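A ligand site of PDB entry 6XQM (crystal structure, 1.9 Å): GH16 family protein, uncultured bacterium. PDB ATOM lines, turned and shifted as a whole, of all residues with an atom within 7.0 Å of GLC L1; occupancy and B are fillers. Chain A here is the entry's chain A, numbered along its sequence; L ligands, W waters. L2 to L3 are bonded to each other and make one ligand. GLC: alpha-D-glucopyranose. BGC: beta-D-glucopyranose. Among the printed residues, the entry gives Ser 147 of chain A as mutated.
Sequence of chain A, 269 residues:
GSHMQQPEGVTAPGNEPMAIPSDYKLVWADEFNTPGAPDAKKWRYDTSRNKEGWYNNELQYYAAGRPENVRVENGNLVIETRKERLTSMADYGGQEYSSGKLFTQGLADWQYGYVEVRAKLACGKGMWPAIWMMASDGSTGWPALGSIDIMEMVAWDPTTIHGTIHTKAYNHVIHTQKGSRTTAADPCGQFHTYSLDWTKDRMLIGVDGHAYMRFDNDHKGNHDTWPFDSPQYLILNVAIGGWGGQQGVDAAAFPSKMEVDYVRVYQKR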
ATOM      1  N   ASN A  56      19.902 -15.379 -30.123  1.00  0.00           N
ATOM      2  CA  ASN A  56      19.767 -13.975 -30.591  1.00  0.00           C
ATOM      3  C   ASN A  56      20.968 -13.529 -31.457  1.00  0.00           C
ATOM      4  O   ASN A  56      21.302 -12.302 -31.436  1.00  0.00           O
ATOM      5  CB  ASN A  56      19.560 -13.041 -29.406  1.00  0.00           C
ATOM      6  CG  ASN A  56      18.528 -13.509 -28.402  1.00  0.00           C
ATOM      7  OD1 ASN A  56      17.358 -13.710 -28.765  1.00  0.00           O
ATOM      8  ND2 ASN A  56      18.945 -13.745 -27.180  1.00  0.00           N
ATOM      9  N   TRP A 128      24.791  -5.280 -24.658  1.00  0.00           N
ATOM     10  CA  TRP A 128      23.380  -5.572 -24.338  1.00  0.00           C
ATOM     11  C   TRP A 128      23.305  -6.089 -22.906  1.00  0.00           C
ATOM     12  O   TRP A 128      23.218  -7.264 -22.679  1.00  0.00           O
ATOM     13  CB  TRP A 128      22.897  -6.561 -25.380  1.00  0.00           C
ATOM     14  CG  TRP A 128      21.481  -7.035 -25.220  1.00  0.00           C
ATOM     15  CD1 TRP A 128      20.522  -6.624 -24.342  1.00  0.00           C
ATOM     16  CD2 TRP A 128      20.868  -8.041 -26.021  1.00  0.00           C
ATOM     17  NE1 TRP A 128      19.336  -7.300 -24.554  1.00  0.00           N
ATOM     18  CE2 TRP A 128      19.525  -8.189 -25.583  1.00  0.00           C
ATOM     19  CE3 TRP A 128      21.330  -8.847 -27.072  1.00  0.00           C
ATOM     20  CZ2 TRP A 128      18.675  -9.157 -26.099  1.00  0.00           C
ATOM     21  CZ3 TRP A 128      20.479  -9.755 -27.640  1.00  0.00           C
ATOM     22  CH2 TRP A 128      19.156  -9.892 -27.166  1.00  0.00           C
ATOM     23  N   TRP A 142      11.364 -22.453 -23.689  1.00  0.00           N
ATOM     24  CA  TRP A 142      11.224 -20.998 -23.959  1.00  0.00           C
ATOM     25  C   TRP A 142      10.487 -20.882 -25.288  1.00  0.00           C
ATOM     26  O   TRP A 142      10.863 -21.571 -26.225  1.00  0.00           O
ATOM     27  CB  TRP A 142      12.584 -20.263 -23.966  1.00  0.00           C
ATOM     28  CG  TRP A 142      12.401 -18.775 -23.993  1.00  0.00           C
ATOM     29  CD1 TRP A 142      12.353 -17.916 -22.943  1.00  0.00           C
ATOM     30  CD2 TRP A 142      12.114 -17.985 -25.152  1.00  0.00           C
ATOM     31  NE1 TRP A 142      12.053 -16.649 -23.357  1.00  0.00           N
ATOM     32  CE2 TRP A 142      11.947 -16.656 -24.714  1.00  0.00           C
ATOM     33  CE3 TRP A 142      12.011 -18.269 -26.517  1.00  0.00           C
ATOM     34  CZ2 TRP A 142      11.644 -15.626 -25.602  1.00  0.00           C
ATOM     35  CZ3 TRP A 142      11.747 -17.255 -27.396  1.00  0.00           C
ATOM     36  CH2 TRP A 142      11.562 -15.953 -26.931  1.00  0.00           C
ATOM     37  N   SER A 147       9.449 -15.625 -18.919  1.00  0.00           N
ATOM     38  CA  SER A 147      10.718 -14.923 -18.602  1.00  0.00           C
ATOM     39  C   SER A 147      10.400 -13.457 -18.325  1.00  0.00           C
ATOM     40  O   SER A 147       9.366 -12.920 -18.872  1.00  0.00           O
ATOM     41  CB  SER A 147      11.749 -15.154 -19.671  1.00  0.00           C
ATOM     42  OG  SER A 147      11.486 -14.389 -20.828  1.00  0.00           O
ATOM     43  N   ASP A 149      12.109  -9.654 -17.997  1.00  0.00           N
ATOM     44  CA  ASP A 149      13.244  -8.716 -18.202  1.00  0.00           C
ATOM     45  C   ASP A 149      13.042  -7.495 -17.305  1.00  0.00           C
ATOM     46  O   ASP A 149      12.283  -6.568 -17.736  1.00  0.00           O
ATOM     47  CB  ASP A 149      13.378  -8.311 -19.684  1.00  0.00           C
ATOM     48  CG  ASP A 149      13.842  -9.464 -20.559  1.00  0.00           C
ATOM     49  OD1 ASP A 149      15.107  -9.727 -20.628  1.00  0.00           O
ATOM     50  OD2 ASP A 149      12.979 -10.139 -21.118  1.00  0.00           O
ATOM     51  N   GLU A 152      16.503  -4.358 -19.652  1.00  0.00           N
ATOM     52  CA  GLU A 152      17.454  -4.491 -20.766  1.00  0.00           C
ATOM     53  C   GLU A 152      17.765  -3.114 -21.320  1.00  0.00           C
ATOM     54  O   GLU A 152      16.870  -2.195 -21.342  1.00  0.00           O
ATOM     55  CB  GLU A 152      16.955  -5.379 -21.907  1.00  0.00           C
ATOM     56  CG  GLU A 152      16.724  -6.831 -21.543  1.00  0.00           C
ATOM     57  CD  GLU A 152      15.989  -7.607 -22.617  1.00  0.00           C
ATOM     58  OE1 GLU A 152      16.646  -8.166 -23.554  1.00  0.00           O
ATOM     59  OE2 GLU A 152      14.737  -7.544 -22.594  1.00  0.00           O
ATOM     60  N   HIS A 162      14.392  -0.868 -21.140  1.00  0.00           N
ATOM     61  CA  HIS A 162      13.283  -1.711 -21.623  1.00  0.00           C
ATOM     62  C   HIS A 162      12.908  -2.672 -20.503  1.00  0.00           C
ATOM     63  O   HIS A 162      13.825  -3.281 -19.907  1.00  0.00           O
ATOM     64  CB  HIS A 162      13.710  -2.444 -22.880  1.00  0.00           C
ATOM     65  CG  HIS A 162      14.139  -1.565 -24.004  1.00  0.00           C
ATOM     66  ND1 HIS A 162      13.301  -1.213 -25.055  1.00  0.00           N
ATOM     67  CD2 HIS A 162      15.356  -1.066 -24.295  1.00  0.00           C
ATOM     68  CE1 HIS A 162      14.013  -0.542 -25.939  1.00  0.00           C
ATOM     69  NE2 HIS A 162      15.279  -0.399 -25.468  1.00  0.00           N
ATOM     70  N   GLY A 163      11.611  -2.813 -20.245  1.00  0.00           N
ATOM     71  CA  GLY A 163      11.126  -3.827 -19.308  1.00  0.00           C
ATOM     72  C   GLY A 163      10.111  -4.653 -20.036  1.00  0.00           C
ATOM     73  O   GLY A 163       9.250  -4.059 -20.803  1.00  0.00           O
ATOM     74  N   THR A 164      10.261  -5.961 -19.988  1.00  0.00           N
ATOM     75  CA  THR A 164       9.554  -6.822 -20.933  1.00  0.00           C
ATOM     76  C   THR A 164       9.280  -8.140 -20.274  1.00  0.00           C
ATOM     77  O   THR A 164      10.133  -8.584 -19.525  1.00  0.00           O
ATOM     78  CB  THR A 164      10.386  -7.035 -22.215  1.00  0.00           C
ATOM     79  OG1 THR A 164      10.915  -5.785 -22.703  1.00  0.00           O
ATOM     80  CG2 THR A 164       9.513  -7.697 -23.255  1.00  0.00           C
ATOM     81  N   ILE A 165       8.125  -8.738 -20.554  1.00  0.00           N
ATOM     82  CA  ILE A 165       7.910 -10.156 -20.211  1.00  0.00           C
ATOM     83  C   ILE A 165       7.614 -10.929 -21.496  1.00  0.00           C
ATOM     84  O   ILE A 165       7.166 -10.345 -22.463  1.00  0.00           O
ATOM     85  CB  ILE A 165       6.850 -10.316 -19.103  1.00  0.00           C
ATOM     86  CG1 ILE A 165       5.432  -9.882 -19.516  1.00  0.00           C
ATOM     87  CG2 ILE A 165       7.365  -9.580 -17.881  1.00  0.00           C
ATOM     88  CD1 ILE A 165       4.687 -10.906 -20.286  1.00  0.00           C
ATOM     89  N   HIS A 166       7.883 -12.218 -21.438  1.00  0.00           N
ATOM     90  CA  HIS A 166       7.692 -13.157 -22.554  1.00  0.00           C
ATOM     91  C   HIS A 166       6.890 -14.351 -22.062  1.00  0.00           C
ATOM     92  O   HIS A 166       7.270 -14.901 -21.008  1.00  0.00           O
ATOM     93  CB  HIS A 166       9.036 -13.581 -23.108  1.00  0.00           C
ATOM     94  CG  HIS A 166       9.830 -12.436 -23.622  1.00  0.00           C
ATOM     95  ND1 HIS A 166       9.733 -12.002 -24.913  1.00  0.00           N
ATOM     96  CD2 HIS A 166      10.680 -11.617 -23.000  1.00  0.00           C
ATOM     97  CE1 HIS A 166      10.545 -10.945 -25.071  1.00  0.00           C
ATOM     98  NE2 HIS A 166      11.138 -10.665 -23.902  1.00  0.00           N
ATOM     99  N   HIS A 172       8.992 -12.183 -28.269  1.00  0.00           N
ATOM    100  CA  HIS A 172       9.655 -11.333 -29.300  1.00  0.00           C
ATOM    101  C   HIS A 172       9.750 -12.100 -30.626  1.00  0.00           C
ATOM    102  O   HIS A 172       9.727 -11.443 -31.674  1.00  0.00           O
ATOM    103  CB  HIS A 172      11.024 -10.807 -28.849  1.00  0.00           C
ATOM    104  CG  HIS A 172      12.031 -11.902 -28.676  1.00  0.00           C
ATOM    105  ND1 HIS A 172      12.725 -12.425 -29.738  1.00  0.00           N
ATOM    106  CD2 HIS A 172      12.473 -12.522 -27.550  1.00  0.00           C
ATOM    107  CE1 HIS A 172      13.574 -13.327 -29.307  1.00  0.00           C
ATOM    108  NE2 HIS A 172      13.404 -13.444 -27.955  1.00  0.00           N
ATOM    109  N   VAL A 173       9.695 -13.419 -30.625  1.00  0.00           N
ATOM    110  CA  VAL A 173       9.844 -14.208 -31.874  1.00  0.00           C
ATOM    111  C   VAL A 173       8.668 -13.923 -32.793  1.00  0.00           C
ATOM    112  O   VAL A 173       8.889 -13.853 -34.025  1.00  0.00           O
ATOM    113  CB  VAL A 173      10.018 -15.708 -31.610  1.00  0.00           C
ATOM    114  CG1 VAL A 173      10.013 -16.474 -32.921  1.00  0.00           C
ATOM    115  CG2 VAL A 173      11.305 -15.929 -30.791  1.00  0.00           C
ATOM    116  N   GLN A 177       5.690  -9.623 -27.602  1.00  0.00           N
ATOM    117  CA  GLN A 177       6.236  -9.396 -26.246  1.00  0.00           C
ATOM    118  C   GLN A 177       5.437  -8.271 -25.567  1.00  0.00           C
ATOM    119  O   GLN A 177       4.936  -7.382 -26.220  1.00  0.00           O
ATOM    120  CB  GLN A 177       7.742  -9.041 -26.277  1.00  0.00           C
ATOM    121  CG  GLN A 177       8.017  -7.675 -26.884  1.00  0.00           C
ATOM    122  CD  GLN A 177       8.358  -7.823 -28.353  1.00  0.00           C
ATOM    123  OE1 GLN A 177       7.762  -8.589 -29.087  1.00  0.00           O
ATOM    124  NE2 GLN A 177       9.429  -7.160 -28.772  1.00  0.00           N
ATOM    125  N   LYS A 178       5.286  -8.370 -24.248  1.00  0.00           N
ATOM    126  CA  LYS A 178       4.586  -7.328 -23.448  1.00  0.00           C
ATOM    127  C   LYS A 178       5.650  -6.443 -22.808  1.00  0.00           C
ATOM    128  O   LYS A 178       6.359  -6.908 -21.877  1.00  0.00           O
ATOM    129  CB  LYS A 178       3.721  -8.013 -22.404  1.00  0.00           C
ATOM    130  CG  LYS A 178       2.544  -8.746 -23.018  1.00  0.00           C
ATOM    131  CD  LYS A 178       1.630  -7.870 -23.776  1.00  0.00           C
ATOM    132  CE  LYS A 178       0.282  -8.509 -23.932  1.00  0.00           C
ATOM    133  NZ  LYS A 178      -0.626  -7.629 -24.678  1.00  0.00           N
ATOM    134  N   GLY A 179       5.812  -5.226 -23.312  1.00  0.00           N
ATOM    135  CA  GLY A 179       6.929  -4.391 -22.865  1.00  0.00           C
ATOM    136  C   GLY A 179       6.599  -2.921 -22.877  1.00  0.00           C
ATOM    137  O   GLY A 179       5.579  -2.488 -23.443  1.00  0.00           O
ATOM    138  N   SER A 180       7.470  -2.185 -22.190  1.00  0.00           N
ATOM    139  CA  SER A 180       7.511  -0.714 -22.196  1.00  0.00           C
ATOM    140  C   SER A 180       8.972  -0.281 -22.125  1.00  0.00           C
ATOM    141  O   SER A 180       9.889  -1.146 -22.040  1.00  0.00           O
ATOM    142  CB  SER A 180       6.690  -0.187 -21.037  1.00  0.00           C
ATOM    143  OG  SER A 180       6.464   1.191 -21.173  1.00  0.00           O
ATOM    144  N   GLY A 242      23.572  -9.328 -31.474  1.00  0.00           N
ATOM    145  CA  GLY A 242      22.096  -9.397 -31.516  1.00  0.00           C
ATOM    146  C   GLY A 242      21.484  -8.005 -31.529  1.00  0.00           C
ATOM    147  O   GLY A 242      21.975  -7.114 -32.253  1.00  0.00           O
ATOM    148  N   TRP A 243      20.524  -7.786 -30.631  1.00  0.00           N
ATOM    149  CA  TRP A 243      19.851  -6.486 -30.385  1.00  0.00           C
ATOM    150  C   TRP A 243      20.861  -5.369 -30.101  1.00  0.00           C
ATOM    151  O   TRP A 243      20.656  -4.282 -30.631  1.00  0.00           O
ATOM    152  CB  TRP A 243      18.857  -6.654 -29.227  1.00  0.00           C
ATOM    153  CG  TRP A 243      17.769  -5.630 -29.213  1.00  0.00           C
ATOM    154  CD1 TRP A 243      17.409  -4.759 -30.186  1.00  0.00           C
ATOM    155  CD2 TRP A 243      16.984  -5.309 -28.060  1.00  0.00           C
ATOM    156  NE1 TRP A 243      16.395  -3.960 -29.746  1.00  0.00           N
ATOM    157  CE2 TRP A 243      16.142  -4.247 -28.427  1.00  0.00           C
ATOM    158  CE3 TRP A 243      16.969  -5.813 -26.767  1.00  0.00           C
ATOM    159  CZ2 TRP A 243      15.237  -3.705 -27.537  1.00  0.00           C
ATOM    160  CZ3 TRP A 243      16.070  -5.265 -25.882  1.00  0.00           C
ATOM    161  CH2 TRP A 243      15.197  -4.243 -26.270  1.00  0.00           C
HETATM  162  C1  GLC L   1      12.593  -7.289 -27.700  1.00  0.00           C
HETATM  163  C2  GLC L   1      12.264  -7.471 -26.193  1.00  0.00           C
HETATM  164  C3  GLC L   1      13.444  -8.048 -25.370  1.00  0.00           C
HETATM  165  C4  GLC L   1      14.208  -9.179 -26.077  1.00  0.00           C
HETATM  166  C5  GLC L   1      14.731  -8.685 -27.422  1.00  0.00           C
HETATM  167  C6  GLC L   1      15.306  -9.905 -28.163  1.00  0.00           C
HETATM  168  O1  GLC L   1      12.356  -6.105 -28.462  1.00  0.00           O
HETATM  169  O2  GLC L   1      11.826  -6.278 -25.524  1.00  0.00           O
HETATM  170  O3  GLC L   1      13.051  -8.513 -24.084  1.00  0.00           O
HETATM  171  O4  GLC L   1      15.273  -9.707 -25.280  1.00  0.00           O
HETATM  172  O5  GLC L   1      13.580  -8.212 -28.171  1.00  0.00           O
HETATM  173  O6  GLC L   1      15.765  -9.505 -29.458  1.00  0.00           O
HETATM  174  C1  GLC L   2      14.685 -11.818 -23.125  1.00  0.00           C
HETATM  175  C2  GLC L   2      14.927 -12.599 -24.370  1.00  0.00           C
HETATM  176  C3  GLC L   2      16.182 -13.516 -24.133  1.00  0.00           C
HETATM  177  C4  GLC L   2      17.479 -12.696 -23.734  1.00  0.00           C
HETATM  178  C5  GLC L   2      17.133 -11.929 -22.459  1.00  0.00           C
HETATM  179  C6  GLC L   2      18.257 -10.992 -21.989  1.00  0.00           C
HETATM  180  O1  GLC L   2      14.132 -12.802 -22.199  1.00  0.00           O
HETATM  181  O2  GLC L   2      13.760 -13.364 -24.615  1.00  0.00           O
HETATM  182  O3  GLC L   2      16.448 -14.268 -25.317  1.00  0.00           O
HETATM  183  O4  GLC L   2      18.689 -13.569 -23.689  1.00  0.00           O
HETATM  184  O5  GLC L   2      15.946 -11.139 -22.694  1.00  0.00           O
HETATM  185  O6  GLC L   2      18.503  -9.848 -22.864  1.00  0.00           O
HETATM  186  C2  BGC L   3      16.180 -16.122 -26.869  1.00  0.00           C
HETATM  187  C3  BGC L   3      15.736 -17.586 -26.988  1.00  0.00           C
HETATM  188  C4  BGC L   3      16.251 -18.419 -25.795  1.00  0.00           C
HETATM  189  C5  BGC L   3      15.894 -17.769 -24.450  1.00  0.00           C
HETATM  190  C6  BGC L   3      16.369 -18.513 -23.211  1.00  0.00           C
HETATM  191  C1  BGC L   3      15.982 -15.581 -25.472  1.00  0.00           C
HETATM  192  O2  BGC L   3      15.510 -15.286 -27.848  1.00  0.00           O
HETATM  193  O3  BGC L   3      16.048 -18.164 -28.253  1.00  0.00           O
HETATM  194  O4  BGC L   3      15.560 -19.639 -25.798  1.00  0.00           O
HETATM  195  O5  BGC L   3      16.432 -16.477 -24.458  1.00  0.00           O
HETATM  196  O6  BGC L   3      17.794 -18.496 -23.283  1.00  0.00           O
HETATM  197  O   HOH W   1      16.617 -11.959 -30.559  1.00  0.00           O
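O1 of GLC L1 lies within hydrogen-bond range of NE2 of Gln 177 (3.1 Å).
The side-chain carboxylate (OD2) of Asp 149 is in hydrogen-bond range of an oxygen (O1) of GLC L2 (3.1 Å).
An oxygen (O3) of GLC L1 is in hydrogen-bond range of the side-chain carboxylate of Asp 149 (3.4 Å).
O3 of GLC L1 lies within hydrogen-bond range of OE2 of Glu 152 (2.4 Å).
OD1 of Asn 56 lies within hydrogen-bond range of O2 of BGC L3.
An oxygen (O1) of GLC L2 sits at hydrogen-bond distance from the side-chain hydroxyl of Ser 147, 3.4 Å away.
An oxygen (O2) of GLC L1 sits at hydrogen-bond distance from the side-chain hydroxyl (OG1) of Thr 164 (3.0 Å).
O6 of GLC L2 lies within hydrogen-bond range of OE1 of Glu 152 (2.6 Å).
A ring nitrogen (NE2) of His 172 sits at hydrogen-bond distance from an oxygen (O2) of BGC L3 (2.8 Å).
An oxygen (O6) of GLC L2 sits at hydrogen-bond distance from the indole nitrogen (NE1) of Trp 128 (3.2 Å).
O3 of GLC L1 is in hydrogen-bond range of NE2 of His 166, 2.9 Å away.
An oxygen (O4) of GLC L1 sits at hydrogen-bond distance from an oxygen (O5) of GLC L2 (3.0 Å).
OE1 of Glu 152 lies within hydrogen-bond range of NE1 of Trp 128 (3.0 Å).
The backbone NH (N) of His 166 sits at hydrogen-bond distance from the backbone carbonyl oxygen (O) of Ser 147 (3.0 Å).
O of Thr 164 is in hydrogen-bond range of N of Asp 149, 2.7 Å away.
A ring nitrogen (NE2) of His 166 lies close to the side-chain carboxylate of Asp 149 (3.4 Å).
ND1 of His 166 lies within hydrogen-bond range of N of His 172 (3.4 Å).
The backbone NH (N) of His 162 lies within hydrogen-bond range of the backbone carbonyl oxygen (O) of Glu 152 (2.8 Å).
CZ2 of Trp 128 touches O4 of GLC L1, at 3.5 Å.
CB of His 172 touches O5 of GLC L1 (3.7 Å).
CE3 of Trp 243 touches C5 of GLC L1 (3.7 Å).
Hydrophobic or aromatic side chains within 4 Å of GLC L1: Trp 128, His 166, His 172 and Trp 243.
Of the 19 residues printed, 8 come within 4 Å of GLC L1.
Water W1 bridges the side-chain amide oxygen of Asn 56 and an oxygen (O6) of GLC L1.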
